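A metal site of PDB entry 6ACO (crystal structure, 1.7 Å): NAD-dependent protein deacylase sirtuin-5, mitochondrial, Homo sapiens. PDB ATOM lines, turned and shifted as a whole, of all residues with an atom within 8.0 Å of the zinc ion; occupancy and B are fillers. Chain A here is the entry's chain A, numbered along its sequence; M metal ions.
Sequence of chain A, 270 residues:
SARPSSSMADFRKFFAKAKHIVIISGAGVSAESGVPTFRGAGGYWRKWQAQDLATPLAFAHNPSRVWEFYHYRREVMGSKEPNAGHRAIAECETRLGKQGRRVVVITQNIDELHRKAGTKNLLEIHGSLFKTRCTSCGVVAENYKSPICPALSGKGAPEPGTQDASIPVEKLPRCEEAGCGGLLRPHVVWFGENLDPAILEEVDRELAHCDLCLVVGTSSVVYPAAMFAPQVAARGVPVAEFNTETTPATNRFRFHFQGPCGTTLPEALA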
ATOM      1  N   ARG A 133     -32.298 -21.380   3.639  1.00  0.00           N
ATOM      2  CA  ARG A 133     -30.928 -21.840   3.931  1.00  0.00           C
ATOM      3  C   ARG A 133     -30.213 -22.152   2.628  1.00  0.00           C
ATOM      4  O   ARG A 133     -30.751 -22.703   1.682  1.00  0.00           O
ATOM      5  CB  ARG A 133     -30.926 -23.043   4.884  1.00  0.00           C
ATOM      6  CG  ARG A 133     -29.525 -23.449   5.309  1.00  0.00           C
ATOM      7  CD  ARG A 133     -29.454 -24.622   6.312  1.00  0.00           C
ATOM      8  NE  ARG A 133     -29.982 -25.913   5.816  1.00  0.00           N
ATOM      9  CZ  ARG A 133     -31.039 -26.597   6.301  1.00  0.00           C
ATOM     10  NH1 ARG A 133     -31.732 -26.172   7.326  1.00  0.00           N
ATOM     11  NH2 ARG A 133     -31.388 -27.767   5.799  1.00  0.00           N
ATOM     12  N   CYS A 134     -28.956 -21.735   2.542  1.00  0.00           N
ATOM     13  CA  CYS A 134     -28.158 -22.011   1.337  1.00  0.00           C
ATOM     14  C   CYS A 134     -27.592 -23.411   1.228  1.00  0.00           C
ATOM     15  O   CYS A 134     -27.002 -23.906   2.216  1.00  0.00           O
ATOM     16  CB  CYS A 134     -26.974 -21.078   1.354  1.00  0.00           C
ATOM     17  SG  CYS A 134     -26.135 -21.205  -0.214  1.00  0.00           S
ATOM     18  N   THR A 135     -27.731 -24.058   0.079  1.00  0.00           N
ATOM     19  CA  THR A 135     -27.222 -25.439  -0.084  1.00  0.00           C
ATOM     20  C   THR A 135     -25.681 -25.555  -0.116  1.00  0.00           C
ATOM     21  O   THR A 135     -25.138 -26.677   0.004  1.00  0.00           O
ATOM     22  CB  THR A 135     -27.887 -26.222  -1.213  1.00  0.00           C
ATOM     23  OG1 THR A 135     -27.620 -25.606  -2.485  1.00  0.00           O
ATOM     24  CG2 THR A 135     -29.400 -26.324  -0.989  1.00  0.00           C
ATOM     25  N   SER A 136     -24.999 -24.393  -0.215  1.00  0.00           N
ATOM     26  CA  SER A 136     -23.542 -24.291  -0.283  1.00  0.00           C
ATOM     27  C   SER A 136     -22.975 -23.652   0.963  1.00  0.00           C
ATOM     28  O   SER A 136     -22.114 -24.199   1.623  1.00  0.00           O
ATOM     29  CB  SER A 136     -23.120 -23.447  -1.512  1.00  0.00           C
ATOM     30  OG  SER A 136     -23.685 -23.990  -2.676  1.00  0.00           O
ATOM     31  N   CYS A 137     -23.433 -22.476   1.281  1.00  0.00           N
ATOM     32  CA  CYS A 137     -22.786 -21.802   2.396  1.00  0.00           C
ATOM     33  C   CYS A 137     -23.459 -22.007   3.751  1.00  0.00           C
ATOM     34  O   CYS A 137     -22.841 -21.711   4.777  1.00  0.00           O
ATOM     35  CB  CYS A 137     -22.521 -20.312   2.116  1.00  0.00           C
ATOM     36  SG  CYS A 137     -23.911 -19.160   2.253  1.00  0.00           S
ATOM     37  N   GLY A 138     -24.659 -22.595   3.808  1.00  0.00           N
ATOM     38  CA  GLY A 138     -25.365 -22.823   5.093  1.00  0.00           C
ATOM     39  C   GLY A 138     -25.977 -21.681   5.914  1.00  0.00           C
ATOM     40  O   GLY A 138     -26.548 -21.912   7.001  1.00  0.00           O
ATOM     41  N   VAL A 139     -25.888 -20.445   5.434  1.00  0.00           N
ATOM     42  CA  VAL A 139     -26.492 -19.325   6.129  1.00  0.00           C
ATOM     43  C   VAL A 139     -28.044 -19.365   6.038  1.00  0.00           C
ATOM     44  O   VAL A 139     -28.630 -19.678   4.988  1.00  0.00           O
ATOM     45  CB  VAL A 139     -26.002 -17.979   5.576  1.00  0.00           C
ATOM     46  CG1 VAL A 139     -26.609 -17.697   4.226  1.00  0.00           C
ATOM     47  CG2 VAL A 139     -26.366 -16.865   6.501  1.00  0.00           C
ATOM     48  N   VAL A 140     -28.640 -19.042   7.172  1.00  0.00           N
ATOM     49  CA  VAL A 140     -30.088 -18.975   7.292  1.00  0.00           C
ATOM     50  C   VAL A 140     -30.501 -17.513   7.204  1.00  0.00           C
ATOM     51  O   VAL A 140     -29.955 -16.712   7.898  1.00  0.00           O
ATOM     52  CB  VAL A 140     -30.515 -19.571   8.633  1.00  0.00           C
ATOM     53  CG1 VAL A 140     -31.998 -19.383   8.896  1.00  0.00           C
ATOM     54  CG2 VAL A 140     -30.179 -21.046   8.650  1.00  0.00           C
ATOM     55  N   ARG A 174     -31.425 -17.669  -4.876  1.00  0.00           N
ATOM     56  CA  ARG A 174     -29.937 -17.775  -4.721  1.00  0.00           C
ATOM     57  C   ARG A 174     -29.402 -17.004  -3.520  1.00  0.00           C
ATOM     58  O   ARG A 174     -30.004 -15.957  -3.145  1.00  0.00           O
ATOM     59  CB  ARG A 174     -29.225 -17.243  -5.992  1.00  0.00           C
ATOM     60  CG  ARG A 174     -29.736 -17.774  -7.325  1.00  0.00           C
ATOM     61  CD  ARG A 174     -29.754 -19.290  -7.469  1.00  0.00           C
ATOM     62  NE  ARG A 174     -28.461 -19.928  -7.261  1.00  0.00           N
ATOM     63  CZ  ARG A 174     -28.067 -21.066  -7.852  1.00  0.00           C
ATOM     64  NH1 ARG A 174     -28.864 -21.737  -8.693  1.00  0.00           N
ATOM     65  NH2 ARG A 174     -26.873 -21.565  -7.585  1.00  0.00           N
ATOM     66  N   CYS A 175     -28.331 -17.501  -2.936  1.00  0.00           N
ATOM     67  CA  CYS A 175     -27.751 -16.850  -1.803  1.00  0.00           C
ATOM     68  C   CYS A 175     -27.371 -15.473  -2.259  1.00  0.00           C
ATOM     69  O   CYS A 175     -26.930 -15.282  -3.361  1.00  0.00           O
ATOM     70  CB  CYS A 175     -26.535 -17.608  -1.264  1.00  0.00           C
ATOM     71  SG  CYS A 175     -26.001 -17.045   0.314  1.00  0.00           S
ATOM     72  N   GLU A 176     -27.577 -14.512  -1.396  1.00  0.00           N
ATOM     73  CA  GLU A 176     -27.137 -13.137  -1.677  1.00  0.00           C
ATOM     74  C   GLU A 176     -25.963 -12.683  -0.828  1.00  0.00           C
ATOM     75  O   GLU A 176     -25.641 -11.504  -0.786  1.00  0.00           O
ATOM     76  CB  GLU A 176     -28.336 -12.191  -1.551  1.00  0.00           C
ATOM     77  CG  GLU A 176     -29.341 -12.472  -2.663  1.00  0.00           C
ATOM     78  CD  GLU A 176     -30.557 -11.550  -2.662  1.00  0.00           C
ATOM     79  OE1 GLU A 176     -30.718 -10.740  -1.688  1.00  0.00           O
ATOM     80  OE2 GLU A 176     -31.345 -11.687  -3.643  1.00  0.00           O
ATOM     81  N   GLU A 177     -25.261 -13.608  -0.177  1.00  0.00           N
ATOM     82  CA  GLU A 177     -24.084 -13.229   0.616  1.00  0.00           C
ATOM     83  C   GLU A 177     -22.885 -13.064  -0.353  1.00  0.00           C
ATOM     84  O   GLU A 177     -22.799 -13.765  -1.356  1.00  0.00           O
ATOM     85  CB  GLU A 177     -23.798 -14.290   1.723  1.00  0.00           C
ATOM     86  CG  GLU A 177     -24.856 -14.391   2.823  1.00  0.00           C
ATOM     87  CD  GLU A 177     -24.914 -13.185   3.774  1.00  0.00           C
ATOM     88  OE1 GLU A 177     -24.309 -12.131   3.508  1.00  0.00           O
ATOM     89  OE2 GLU A 177     -25.603 -13.293   4.817  1.00  0.00           O
ATOM     90  N   ALA A 178     -21.992 -12.131  -0.043  1.00  0.00           N
ATOM     91  CA  ALA A 178     -20.787 -11.860  -0.876  1.00  0.00           C
ATOM     92  C   ALA A 178     -20.093 -13.167  -1.154  1.00  0.00           C
ATOM     93  O   ALA A 178     -19.693 -13.920  -0.206  1.00  0.00           O
ATOM     94  CB  ALA A 178     -19.816 -10.908  -0.163  1.00  0.00           C
ATOM     95  N   GLY A 179     -20.006 -13.486  -2.433  1.00  0.00           N
ATOM     96  CA  GLY A 179     -19.131 -14.587  -2.850  1.00  0.00           C
ATOM     97  C   GLY A 179     -19.677 -15.994  -2.760  1.00  0.00           C
ATOM     98  O   GLY A 179     -18.917 -16.938  -2.964  1.00  0.00           O
ATOM     99  N   CYS A 180     -21.015 -16.124  -2.507  1.00  0.00           N
ATOM    100  CA  CYS A 180     -21.643 -17.485  -2.568  1.00  0.00           C
ATOM    101  C   CYS A 180     -22.465 -17.716  -3.799  1.00  0.00           C
ATOM    102  O   CYS A 180     -22.082 -18.560  -4.596  1.00  0.00           O
ATOM    103  CB  CYS A 180     -22.485 -17.911  -1.353  1.00  0.00           C
ATOM    104  SG  CYS A 180     -23.203 -19.575  -1.579  1.00  0.00           S
ATOM    105  N   GLY A 181     -23.603 -17.025  -3.986  1.00  0.00           N
ATOM    106  CA  GLY A 181     -24.555 -17.417  -5.045  1.00  0.00           C
ATOM    107  C   GLY A 181     -25.060 -18.874  -5.093  1.00  0.00           C
ATOM    108  O   GLY A 181     -25.542 -19.327  -6.136  1.00  0.00           O
ATOM    109  N   GLY A 182     -24.992 -19.598  -3.953  1.00  0.00           N
ATOM    110  CA  GLY A 182     -25.593 -20.965  -3.854  1.00  0.00           C
ATOM    111  C   GLY A 182     -27.083 -21.051  -4.210  1.00  0.00           C
ATOM    112  O   GLY A 182     -27.767 -20.058  -4.252  1.00  0.00           O
ATOM    113  N   LEU A 183     -27.578 -22.238  -4.469  1.00  0.00           N
ATOM    114  CA  LEU A 183     -28.987 -22.525  -4.457  1.00  0.00           C
ATOM    115  C   LEU A 183     -29.468 -22.473  -3.016  1.00  0.00           C
ATOM    116  O   LEU A 183     -28.860 -23.012  -2.097  1.00  0.00           O
ATOM    117  CB  LEU A 183     -29.328 -23.851  -5.114  1.00  0.00           C
ATOM    118  CG  LEU A 183     -30.782 -24.288  -5.231  1.00  0.00           C
ATOM    119  CD1 LEU A 183     -31.694 -23.233  -5.844  1.00  0.00           C
ATOM    120  CD2 LEU A 183     -30.957 -25.596  -5.980  1.00  0.00           C
ATOM    121  N   LEU A 184     -30.533 -21.700  -2.799  1.00  0.00           N
ATOM    122  CA  LEU A 184     -31.271 -21.753  -1.545  1.00  0.00           C
ATOM    123  C   LEU A 184     -32.324 -22.866  -1.583  1.00  0.00           C
ATOM    124  O   LEU A 184     -32.844 -23.249  -2.608  1.00  0.00           O
ATOM    125  CB  LEU A 184     -31.956 -20.397  -1.272  1.00  0.00           C
ATOM    126  CG  LEU A 184     -31.082 -19.153  -1.144  1.00  0.00           C
ATOM    127  CD1 LEU A 184     -31.978 -17.944  -0.854  1.00  0.00           C
ATOM    128  CD2 LEU A 184     -29.982 -19.202  -0.070  1.00  0.00           C
HETATM  129 ZN    ZN M   1     -24.792 -19.267   0.199  1.00  0.00          ZN
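The backbone NH (N) of Cys 134 lies within hydrogen-bond range of the backbone carbonyl oxygen (O) of Val 139. The backbone NH (N) of Ser 136 sits close to the side-chain sulfur (SG) of Cys 134 (3.4 Å). The backbone carbonyl oxygen of Leu 183 lies close to the side-chain sulfur of Cys 134. The backbone NH (N) of Gly 182 sits close to the side-chain sulfur (SG) of Cys 180, 3.0 Å away. The backbone NH (N) of Cys 175 is in hydrogen-bond range of the backbone carbonyl oxygen (O) of Gly 182, at 2.9 Å. The side-chain sulfur (SG) of Cys 175 lies close to the backbone NH (N) of Glu 177 (3.5 Å).
The zinc ion is bound by SG of Cys 137 (2.2 Å), SG of Cys 134 (2.4 Å), SG of Cys 180 (2.4 Å) and SG of Cys 175 (2.5 Å).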
